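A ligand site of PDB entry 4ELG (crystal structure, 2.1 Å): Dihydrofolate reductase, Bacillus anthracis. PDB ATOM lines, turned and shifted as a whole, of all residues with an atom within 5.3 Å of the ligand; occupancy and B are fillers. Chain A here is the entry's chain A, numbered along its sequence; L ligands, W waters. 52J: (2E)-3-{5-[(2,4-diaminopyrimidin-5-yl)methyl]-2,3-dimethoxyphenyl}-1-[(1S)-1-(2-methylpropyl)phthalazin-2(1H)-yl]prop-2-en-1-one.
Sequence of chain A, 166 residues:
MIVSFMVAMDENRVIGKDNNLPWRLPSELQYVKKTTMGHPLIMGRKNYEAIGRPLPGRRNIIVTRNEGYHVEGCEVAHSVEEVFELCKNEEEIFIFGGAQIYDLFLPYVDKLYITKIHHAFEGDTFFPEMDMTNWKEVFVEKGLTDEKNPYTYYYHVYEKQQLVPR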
ATOM      1  N   MET A   6      -3.855 -30.467  -3.721  1.00  0.00           N
ATOM      2  CA  MET A   6      -4.180 -30.369  -2.316  1.00  0.00           C
ATOM      3  C   MET A   6      -5.689 -30.231  -2.234  1.00  0.00           C
ATOM      4  O   MET A   6      -6.271 -29.289  -2.787  1.00  0.00           O
ATOM      5  CB  MET A   6      -3.496 -29.156  -1.674  1.00  0.00           C
ATOM      6  CG  MET A   6      -4.041 -28.770  -0.309  1.00  0.00           C
ATOM      7  SD  MET A   6      -3.720 -30.061   0.923  1.00  0.00           S
ATOM      8  CE  MET A   6      -1.933 -29.981   1.088  1.00  0.00           C
ATOM      9  N   VAL A   7      -6.343 -31.178  -1.562  1.00  0.00           N
ATOM     10  CA  VAL A   7      -7.803 -31.185  -1.555  1.00  0.00           C
ATOM     11  C   VAL A   7      -8.406 -31.668  -0.234  1.00  0.00           C
ATOM     12  O   VAL A   7      -7.885 -32.589   0.423  1.00  0.00           O
ATOM     13  CB  VAL A   7      -8.376 -31.972  -2.786  1.00  0.00           C
ATOM     14  CG1 VAL A   7      -7.980 -33.410  -2.720  1.00  0.00           C
ATOM     15  CG2 VAL A   7      -9.896 -31.828  -2.897  1.00  0.00           C
ATOM     16  N   ALA A   8      -9.498 -31.028   0.168  1.00  0.00           N
ATOM     17  CA  ALA A   8     -10.309 -31.516   1.277  1.00  0.00           C
ATOM     18  C   ALA A   8     -11.727 -31.753   0.763  1.00  0.00           C
ATOM     19  O   ALA A   8     -12.366 -30.832   0.231  1.00  0.00           O
ATOM     20  CB  ALA A   8     -10.316 -30.509   2.421  1.00  0.00           C
ATOM     21  N   ILE A  15     -16.430 -30.231  -2.412  1.00  0.00           N
ATOM     22  CA  ILE A  15     -15.322 -29.378  -1.978  1.00  0.00           C
ATOM     23  C   ILE A  15     -15.781 -27.937  -1.758  1.00  0.00           C
ATOM     24  O   ILE A  15     -15.014 -27.084  -1.312  1.00  0.00           O
ATOM     25  CB  ILE A  15     -14.178 -29.357  -3.016  1.00  0.00           C
ATOM     26  CG1 ILE A  15     -14.687 -28.813  -4.362  1.00  0.00           C
ATOM     27  CG2 ILE A  15     -13.563 -30.756  -3.174  1.00  0.00           C
ATOM     28  CD1 ILE A  15     -13.596 -28.759  -5.463  1.00  0.00           C
ATOM     29  N   ASN A  19     -19.301 -21.149  -2.973  1.00  0.00           N
ATOM     30  CA  ASN A  19     -17.949 -20.611  -2.830  1.00  0.00           C
ATOM     31  C   ASN A  19     -17.489 -20.558  -1.364  1.00  0.00           C
ATOM     32  O   ASN A  19     -16.926 -19.550  -0.919  1.00  0.00           O
ATOM     33  CB  ASN A  19     -17.823 -19.236  -3.481  1.00  0.00           C
ATOM     34  CG  ASN A  19     -18.370 -19.220  -4.899  1.00  0.00           C
ATOM     35  OD1 ASN A  19     -17.972 -20.038  -5.738  1.00  0.00           O
ATOM     36  ND2 ASN A  19     -19.294 -18.286  -5.168  1.00  0.00           N
ATOM     37  N   ASN A  20     -17.726 -21.631  -0.636  1.00  0.00           N
ATOM     38  CA  ASN A  20     -17.281 -21.746   0.747  1.00  0.00           C
ATOM     39  C   ASN A  20     -17.033 -23.193   1.113  1.00  0.00           C
ATOM     40  O   ASN A  20     -17.465 -24.106   0.404  1.00  0.00           O
ATOM     41  CB  ASN A  20     -18.294 -21.099   1.699  1.00  0.00           C
ATOM     42  CG  ASN A  20     -18.148 -19.598   1.776  1.00  0.00           C
ATOM     43  OD1 ASN A  20     -19.068 -18.851   1.438  1.00  0.00           O
ATOM     44  ND2 ASN A  20     -16.975 -19.135   2.211  1.00  0.00           N
ATOM     45  N   LEU A  21     -16.325 -23.433   2.218  1.00  0.00           N
ATOM     46  CA  LEU A  21     -16.230 -24.791   2.745  1.00  0.00           C
ATOM     47  C   LEU A  21     -17.490 -25.050   3.552  1.00  0.00           C
ATOM     48  O   LEU A  21     -17.956 -24.159   4.267  1.00  0.00           O
ATOM     49  CB  LEU A  21     -15.002 -24.991   3.608  1.00  0.00           C
ATOM     50  CG  LEU A  21     -13.655 -24.955   2.877  1.00  0.00           C
ATOM     51  CD1 LEU A  21     -12.519 -25.048   3.895  1.00  0.00           C
ATOM     52  CD2 LEU A  21     -13.550 -26.063   1.805  1.00  0.00           C
ATOM     53  N   PRO A  26     -10.381 -26.110  11.613  1.00  0.00           N
ATOM     54  CA  PRO A  26      -9.135 -25.332  11.690  1.00  0.00           C
ATOM     55  C   PRO A  26      -7.890 -26.215  11.636  1.00  0.00           C
ATOM     56  O   PRO A  26      -6.864 -25.835  11.028  1.00  0.00           O
ATOM     57  CB  PRO A  26      -9.191 -24.668  13.086  1.00  0.00           C
ATOM     58  CG  PRO A  26     -10.612 -24.806  13.543  1.00  0.00           C
ATOM     59  CD  PRO A  26     -11.245 -25.937  12.801  1.00  0.00           C
ATOM     60  N   GLU A  28      -7.476 -29.023  10.102  1.00  0.00           N
ATOM     61  CA  GLU A  28      -7.263 -29.397   8.705  1.00  0.00           C
ATOM     62  C   GLU A  28      -6.459 -28.312   7.980  1.00  0.00           C
ATOM     63  O   GLU A  28      -5.482 -28.604   7.306  1.00  0.00           O
ATOM     64  CB  GLU A  28      -8.590 -29.618   7.985  1.00  0.00           C
ATOM     65  CG  GLU A  28      -8.480 -30.609   6.841  1.00  0.00           C
ATOM     66  CD  GLU A  28      -8.020 -29.988   5.514  1.00  0.00           C
ATOM     67  OE1 GLU A  28      -8.497 -28.870   5.171  1.00  0.00           O
ATOM     68  OE2 GLU A  28      -7.232 -30.642   4.783  1.00  0.00           O
ATOM     69  N   LEU A  29      -6.874 -27.060   8.136  1.00  0.00           N
ATOM     70  CA  LEU A  29      -6.193 -25.947   7.494  1.00  0.00           C
ATOM     71  C   LEU A  29      -4.759 -25.780   8.020  1.00  0.00           C
ATOM     72  O   LEU A  29      -3.833 -25.425   7.255  1.00  0.00           O
ATOM     73  CB  LEU A  29      -6.994 -24.655   7.643  1.00  0.00           C
ATOM     74  CG  LEU A  29      -8.400 -24.772   7.024  1.00  0.00           C
ATOM     75  CD1 LEU A  29      -9.224 -23.478   7.243  1.00  0.00           C
ATOM     76  CD2 LEU A  29      -8.287 -25.115   5.530  1.00  0.00           C
ATOM     77  N   GLN A  30      -4.553 -26.061   9.307  1.00  0.00           N
ATOM     78  CA  GLN A  30      -3.199 -26.092   9.852  1.00  0.00           C
ATOM     79  C   GLN A  30      -2.366 -27.181   9.157  1.00  0.00           C
ATOM     80  O   GLN A  30      -1.173 -27.008   8.943  1.00  0.00           O
ATOM     81  CB  GLN A  30      -3.187 -26.286  11.380  1.00  0.00           C
ATOM     82  CG  GLN A  30      -3.760 -25.101  12.175  1.00  0.00           C
ATOM     83  CD  GLN A  30      -4.243 -25.509  13.569  1.00  0.00           C
ATOM     84  OE1 GLN A  30      -4.009 -26.638  14.021  1.00  0.00           O
ATOM     85  NE2 GLN A  30      -4.928 -24.594  14.262  1.00  0.00           N
ATOM     86  N   VAL A  32      -2.814 -28.181   6.033  1.00  0.00           N
ATOM     87  CA  VAL A  32      -2.552 -27.549   4.748  1.00  0.00           C
ATOM     88  C   VAL A  32      -1.398 -26.552   4.842  1.00  0.00           C
ATOM     89  O   VAL A  32      -0.489 -26.553   3.994  1.00  0.00           O
ATOM     90  CB  VAL A  32      -3.796 -26.837   4.213  1.00  0.00           C
ATOM     91  CG1 VAL A  32      -3.468 -26.046   2.950  1.00  0.00           C
ATOM     92  CG2 VAL A  32      -4.898 -27.836   3.947  1.00  0.00           C
ATOM     93  N   LYS A  33      -1.420 -25.710   5.878  1.00  0.00           N
ATOM     94  CA  LYS A  33      -0.368 -24.721   6.023  1.00  0.00           C
ATOM     95  C   LYS A  33       0.988 -25.399   6.182  1.00  0.00           C
ATOM     96  O   LYS A  33       1.937 -25.048   5.470  1.00  0.00           O
ATOM     97  CB  LYS A  33      -0.629 -23.778   7.206  1.00  0.00           C
ATOM     98  CG  LYS A  33       0.477 -22.722   7.364  1.00  0.00           C
ATOM     99  CD  LYS A  33       0.196 -21.790   8.545  1.00  0.00           C
ATOM    100  CE  LYS A  33       1.295 -20.742   8.723  1.00  0.00           C
ATOM    101  NZ  LYS A  33       0.984 -19.845   9.883  1.00  0.00           N
ATOM    102  N   THR A  36       2.115 -27.218   2.796  1.00  0.00           N
ATOM    103  CA  THR A  36       2.434 -26.414   1.613  1.00  0.00           C
ATOM    104  C   THR A  36       3.530 -25.377   1.826  1.00  0.00           C
ATOM    105  O   THR A  36       3.914 -24.670   0.899  1.00  0.00           O
ATOM    106  CB  THR A  36       1.213 -25.669   1.070  1.00  0.00           C
ATOM    107  OG1 THR A  36       0.682 -24.813   2.096  1.00  0.00           O
ATOM    108  CG2 THR A  36       0.141 -26.639   0.590  1.00  0.00           C
ATOM    109  N   LEU A  41       1.012 -22.035  -3.983  1.00  0.00           N
ATOM    110  CA  LEU A  41      -0.379 -22.471  -4.020  1.00  0.00           C
ATOM    111  C   LEU A  41      -0.957 -21.983  -5.330  1.00  0.00           C
ATOM    112  O   LEU A  41      -0.884 -20.794  -5.648  1.00  0.00           O
ATOM    113  CB  LEU A  41      -1.187 -21.829  -2.884  1.00  0.00           C
ATOM    114  CG  LEU A  41      -0.807 -22.248  -1.471  1.00  0.00           C
ATOM    115  CD1 LEU A  41      -1.822 -21.673  -0.458  1.00  0.00           C
ATOM    116  CD2 LEU A  41      -0.772 -23.759  -1.405  1.00  0.00           C
ATOM    117  N   ASN A  47     -11.852 -19.481  -5.977  1.00  0.00           N
ATOM    118  CA  ASN A  47     -11.254 -20.105  -4.812  1.00  0.00           C
ATOM    119  C   ASN A  47     -10.505 -19.049  -4.011  1.00  0.00           C
ATOM    120  O   ASN A  47     -10.704 -18.936  -2.800  1.00  0.00           O
ATOM    121  CB  ASN A  47     -10.300 -21.241  -5.222  1.00  0.00           C
ATOM    122  CG  ASN A  47     -10.377 -22.457  -4.303  1.00  0.00           C
ATOM    123  OD1 ASN A  47     -11.465 -22.915  -3.949  1.00  0.00           O
ATOM    124  ND2 ASN A  47      -9.221 -22.992  -3.932  1.00  0.00           N
ATOM    125  N   ALA A  50     -12.884 -16.784  -2.224  1.00  0.00           N
ATOM    126  CA  ALA A  50     -13.601 -17.488  -1.156  1.00  0.00           C
ATOM    127  C   ALA A  50     -12.782 -17.430   0.125  1.00  0.00           C
ATOM    128  O   ALA A  50     -13.326 -17.338   1.236  1.00  0.00           O
ATOM    129  CB  ALA A  50     -13.877 -18.928  -1.562  1.00  0.00           C
ATOM    130  N   ILE A  51     -11.462 -17.478  -0.032  1.00  0.00           N
ATOM    131  CA  ILE A  51     -10.518 -17.356   1.067  1.00  0.00           C
ATOM    132  C   ILE A  51     -10.388 -15.877   1.454  1.00  0.00           C
ATOM    133  O   ILE A  51     -10.196 -15.538   2.625  1.00  0.00           O
ATOM    134  CB  ILE A  51      -9.152 -17.946   0.653  1.00  0.00           C
ATOM    135  CG1 ILE A  51      -9.354 -19.371   0.127  1.00  0.00           C
ATOM    136  CG2 ILE A  51      -8.187 -17.925   1.830  1.00  0.00           C
ATOM    137  CD1 ILE A  51      -8.132 -19.976  -0.514  1.00  0.00           C
ATOM    138  N   ARG A  53      -8.215 -13.539   1.098  1.00  0.00           N
ATOM    139  CA  ARG A  53      -6.924 -12.892   1.333  1.00  0.00           C
ATOM    140  C   ARG A  53      -5.755 -13.772   0.877  1.00  0.00           C
ATOM    141  O   ARG A  53      -5.926 -14.977   0.680  1.00  0.00           O
ATOM    142  CB  ARG A  53      -6.773 -12.469   2.818  1.00  0.00           C
ATOM    143  CG  ARG A  53      -6.226 -13.533   3.753  1.00  0.00           C
ATOM    144  CD  ARG A  53      -7.265 -14.609   4.088  1.00  0.00           C
ATOM    145  NE  ARG A  53      -6.756 -15.570   5.069  1.00  0.00           N
ATOM    146  CZ  ARG A  53      -7.418 -16.647   5.466  1.00  0.00           C
ATOM    147  NH1 ARG A  53      -8.626 -16.922   4.980  1.00  0.00           N
ATOM    148  NH2 ARG A  53      -6.876 -17.467   6.371  1.00  0.00           N
ATOM    149  N   LEU A  55      -2.719 -16.126   1.341  1.00  0.00           N
ATOM    150  CA  LEU A  55      -2.186 -16.991   2.388  1.00  0.00           C
ATOM    151  C   LEU A  55      -0.662 -16.780   2.498  1.00  0.00           C
ATOM    152  O   LEU A  55       0.091 -17.134   1.578  1.00  0.00           O
ATOM    153  CB  LEU A  55      -2.547 -18.447   2.118  1.00  0.00           C
ATOM    154  CG  LEU A  55      -4.057 -18.650   2.042  1.00  0.00           C
ATOM    155  CD1 LEU A  55      -4.438 -20.088   1.658  1.00  0.00           C
ATOM    156  CD2 LEU A  55      -4.721 -18.235   3.359  1.00  0.00           C
ATOM    157  N   PRO A  56      -0.214 -16.184   3.605  1.00  0.00           N
ATOM    158  CA  PRO A  56       1.161 -15.708   3.741  1.00  0.00           C
ATOM    159  C   PRO A  56       2.175 -16.845   3.818  1.00  0.00           C
ATOM    160  O   PRO A  56       1.796 -17.975   4.136  1.00  0.00           O
ATOM    161  CB  PRO A  56       1.136 -14.916   5.059  1.00  0.00           C
ATOM    162  CG  PRO A  56       0.010 -15.539   5.844  1.00  0.00           C
ATOM    163  CD  PRO A  56      -1.014 -15.955   4.825  1.00  0.00           C
ATOM    164  N   ARG A  58       3.687 -18.083   1.358  1.00  0.00           N
ATOM    165  CA  ARG A  58       3.576 -18.883   0.140  1.00  0.00           C
ATOM    166  C   ARG A  58       3.441 -17.997  -1.102  1.00  0.00           C
ATOM    167  O   ARG A  58       2.924 -16.875  -1.030  1.00  0.00           O
ATOM    168  CB  ARG A  58       2.380 -19.831   0.236  1.00  0.00           C
ATOM    169  CG  ARG A  58       2.681 -21.127   0.972  1.00  0.00           C
ATOM    170  CD  ARG A  58       1.738 -21.328   2.144  1.00  0.00           C
ATOM    171  NE  ARG A  58       2.392 -22.029   3.251  1.00  0.00           N
ATOM    172  CZ  ARG A  58       2.896 -21.418   4.324  1.00  0.00           C
ATOM    173  NH1 ARG A  58       2.799 -20.106   4.437  1.00  0.00           N
ATOM    174  NH2 ARG A  58       3.481 -22.109   5.295  1.00  0.00           N
ATOM    175  N   ILE A  95      -1.804 -27.494  -6.366  1.00  0.00           N
ATOM    176  CA  ILE A  95      -3.034 -27.097  -7.010  1.00  0.00           C
ATOM    177  C   ILE A  95      -4.076 -27.083  -5.888  1.00  0.00           C
ATOM    178  O   ILE A  95      -4.385 -28.133  -5.286  1.00  0.00           O
ATOM    179  CB  ILE A  95      -3.398 -28.048  -8.138  1.00  0.00           C
ATOM    180  CG1 ILE A  95      -2.174 -28.278  -9.041  1.00  0.00           C
ATOM    181  CG2 ILE A  95      -4.597 -27.495  -8.911  1.00  0.00           C
ATOM    182  CD1 ILE A  95      -1.491 -27.003  -9.536  1.00  0.00           C
ATOM    183  N   PHE A  96      -4.578 -25.889  -5.609  1.00  0.00           N
ATOM    184  CA  PHE A  96      -5.356 -25.610  -4.410  1.00  0.00           C
ATOM    185  C   PHE A  96      -6.840 -25.612  -4.678  1.00  0.00           C
ATOM    186  O   PHE A  96      -7.677 -25.480  -3.767  1.00  0.00           O
ATOM    187  CB  PHE A  96      -4.951 -24.262  -3.823  1.00  0.00           C
ATOM    188  CG  PHE A  96      -5.145 -24.183  -2.360  1.00  0.00           C
ATOM    189  CD1 PHE A  96      -4.742 -25.233  -1.541  1.00  0.00           C
ATOM    190  CD2 PHE A  96      -5.739 -23.075  -1.777  1.00  0.00           C
ATOM    191  CE1 PHE A  96      -4.929 -25.180  -0.160  1.00  0.00           C
ATOM    192  CE2 PHE A  96      -5.924 -23.009  -0.394  1.00  0.00           C
ATOM    193  CZ  PHE A  96      -5.518 -24.073   0.415  1.00  0.00           C
ATOM    194  N   GLY A  97      -7.175 -25.752  -5.942  1.00  0.00           N
ATOM    195  CA  GLY A  97      -8.553 -25.934  -6.268  1.00  0.00           C
ATOM    196  C   GLY A  97      -9.209 -24.797  -6.987  1.00  0.00           C
ATOM    197  O   GLY A  97      -8.588 -23.780  -7.364  1.00  0.00           O
ATOM    198  N   TYR A 102      -8.404 -27.960 -10.838  1.00  0.00           N
ATOM    199  CA  TYR A 102      -7.976 -29.356 -10.798  1.00  0.00           C
ATOM    200  C   TYR A 102      -8.016 -30.000 -12.202  1.00  0.00           C
ATOM    201  O   TYR A 102      -7.094 -30.727 -12.577  1.00  0.00           O
ATOM    202  CB  TYR A 102      -8.819 -30.187  -9.844  1.00  0.00           C
ATOM    203  CG  TYR A 102      -8.648 -29.809  -8.381  1.00  0.00           C
ATOM    204  CD1 TYR A 102      -7.376 -29.657  -7.835  1.00  0.00           C
ATOM    205  CD2 TYR A 102      -9.749 -29.585  -7.562  1.00  0.00           C
ATOM    206  CE1 TYR A 102      -7.212 -29.312  -6.487  1.00  0.00           C
ATOM    207  CE2 TYR A 102      -9.586 -29.240  -6.215  1.00  0.00           C
ATOM    208  CZ  TYR A 102      -8.324 -29.112  -5.688  1.00  0.00           C
ATOM    209  OH  TYR A 102      -8.174 -28.748  -4.363  1.00  0.00           O
ATOM    210  N   THR A 115      -7.613 -34.768   1.739  1.00  0.00           N
ATOM    211  CA  THR A 115      -8.248 -34.903   3.058  1.00  0.00           C
ATOM    212  C   THR A 115      -9.647 -35.436   2.831  1.00  0.00           C
ATOM    213  O   THR A 115     -10.422 -34.849   2.056  1.00  0.00           O
ATOM    214  CB  THR A 115      -8.308 -33.559   3.814  1.00  0.00           C
ATOM    215  OG1 THR A 115      -6.974 -33.055   4.019  1.00  0.00           O
ATOM    216  CG2 THR A 115      -9.013 -33.746   5.182  1.00  0.00           C
HETATM  217  N01 52J L   1      -7.446 -27.091  -1.623  1.00  0.00           N
HETATM  218  C02 52J L   1      -7.771 -27.268  -0.167  1.00  0.00           C
HETATM  219  C03 52J L   1      -8.556 -26.322   0.491  1.00  0.00           C
HETATM  220  C04 52J L   1      -9.068 -25.136  -0.261  1.00  0.00           C
HETATM  221  C05 52J L   1      -9.623 -24.043   0.709  1.00  0.00           C
HETATM  222  C06 52J L   1     -10.910 -23.460   0.452  1.00  0.00           C
HETATM  223  C07 52J L   1     -11.421 -22.470   1.307  1.00  0.00           C
HETATM  224  O08 52J L   1     -12.642 -21.914   1.049  1.00  0.00           O
HETATM  225  C09 52J L   1     -13.558 -22.618   0.186  1.00  0.00           C
HETATM  226  C10 52J L   1     -10.671 -22.041   2.411  1.00  0.00           C
HETATM  227  O11 52J L   1     -11.178 -21.065   3.255  1.00  0.00           O
HETATM  228  C12 52J L   1     -11.653 -21.432   4.556  1.00  0.00           C
HETATM  229  C13 52J L   1      -9.411 -22.612   2.672  1.00  0.00           C
HETATM  230  O30 52J L   1      -7.009 -20.369   5.541  1.00  0.00           O
HETATM  231  C31 52J L   1      -8.888 -23.630   1.790  1.00  0.00           C
HETATM  232  C32 52J L   1      -8.844 -26.514   1.888  1.00  0.00           C
HETATM  233  N33 52J L   1      -8.344 -27.609   2.519  1.00  0.00           N
HETATM  234  C34 52J L   1      -7.595 -28.495   1.847  1.00  0.00           C
HETATM  235  N35 52J L   1      -7.078 -29.653   2.540  1.00  0.00           N
HETATM  236  N36 52J L   1      -7.296 -28.335   0.508  1.00  0.00           N
HETATM  237  C14 52J L   1      -8.582 -22.143   3.906  1.00  0.00           C
HETATM  238  C15 52J L   1      -7.203 -21.889   3.789  1.00  0.00           C
HETATM  239  C16 52J L   1      -6.470 -21.219   4.902  1.00  0.00           C
HETATM  240  N17 52J L   1      -5.132 -21.601   5.218  1.00  0.00           N
HETATM  241  N18 52J L   1      -4.503 -22.561   4.510  1.00  0.00           N
HETATM  242  C19 52J L   1      -3.271 -22.121   3.914  1.00  0.00           C
HETATM  243  C20 52J L   1      -4.433 -20.954   6.282  1.00  0.00           C
HETATM  244  C21 52J L   1      -4.412 -21.880   7.504  1.00  0.00           C
HETATM  245  C22 52J L   1      -3.920 -21.275   8.863  1.00  0.00           C
HETATM  246  C23 52J L   1      -4.941 -20.393   9.536  1.00  0.00           C
HETATM  247  C24 52J L   1      -3.023 -20.628   5.903  1.00  0.00           C
HETATM  248  C25 52J L   1      -2.476 -21.188   4.762  1.00  0.00           C
HETATM  249  C26 52J L   1      -1.141 -20.885   4.390  1.00  0.00           C
HETATM  250  C27 52J L   1      -0.373 -19.998   5.182  1.00  0.00           C
HETATM  251  C28 52J L   1      -0.921 -19.442   6.310  1.00  0.00           C
HETATM  252  C29 52J L   1      -2.269 -19.751   6.685  1.00  0.00           C
HETATM  253  C37 52J L   1      -3.265 -22.360   9.852  1.00  0.00           C
HETATM  254  O   HOH W   1      -6.659 -23.093  10.753  1.00  0.00           O
HETATM  255  O   HOH W   2      -0.996 -23.505  11.945  1.00  0.00           O
HETATM  256  O   HOH W   3      -8.553 -19.806   8.157  1.00  0.00           O
HETATM  257  O   HOH W   4     -10.750 -28.809  -0.992  1.00  0.00           O
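The side-chain carboxylate (OE2) of Glu 28 is in hydrogen-bond range of a nitrogen (N35) of the ligand.
A nitrogen (N01) of the ligand is in hydrogen-bond range of the backbone carbonyl oxygen of Phe 96 (2.7 Å).
N01 of the ligand sits at hydrogen-bond distance from O of Met 6, 2.8 Å away.
SD of Met 6 sits at hydrogen-bond distance from N35 of the ligand, 3.7 Å away.
NH2 of Arg 53 is in hydrogen-bond range of O30 of the ligand (3.0 Å).
A nitrogen (N01) of the ligand sits at hydrogen-bond distance from the side-chain hydroxyl of Tyr 102 (3.3 Å).
The backbone NH (N) of Ala 8 is in hydrogen-bond range of a nitrogen (N36) of the ligand (3.5 Å).
OE2 of Glu 28 sits at hydrogen-bond distance from OG1 of Thr 115 (2.5 Å).
The side-chain amide nitrogen (ND2) of Asn 47 sits at hydrogen-bond distance from the backbone carbonyl oxygen (O) of Phe 96 (2.9 Å).
OH of Tyr 102 is in hydrogen-bond range of O of Met 6 (2.5 Å).
The backbone carbonyl oxygen (O) of Ile 51 is in hydrogen-bond range of the guanidinium group (NH1) of Arg 53, at 3.2 Å.
O of Val 32 is in hydrogen-bond range of OG1 of Thr 36 (2.8 Å).
The guanidinium group (NH2) of Arg 58 is in hydrogen-bond range of the backbone carbonyl oxygen (O) of Lys 33, 3.3 Å away.
The guanidinium group (NE) of Arg 58 sits at hydrogen-bond distance from the side-chain hydroxyl (OG1) of Thr 36 (3.5 Å).
The backbone carbonyl oxygen of Val 7 lies within hydrogen-bond range of the backbone NH of Thr 115, at 2.6 Å.
Residues that only touch the ligand: Val 7, Asn 20, Leu 21, Leu 29, Gln 30, Val 32, Lys 33, Ile 51, Leu 55, Pro 56, Arg 58 and Thr 115.
Hydrophobic or aromatic side chains within 4 Å of the ligand: Met 6, Ala 8, Leu 21, Leu 29, Val 32, Ile 51, Leu 55, Pro 56 and Phe 96.
Of the 27 residues printed, 18 come within 4 Å of the ligand.
Along chain A the residues within 4 Å of the ligand span positions 6 to 115.
The nearest printed residue that does not touch the ligand is Ala 50 (4.1 Å).
Water W3 lies within hydrogen-bond range of an oxygen (O30) of the ligand and the guanidinium group of Arg 53.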
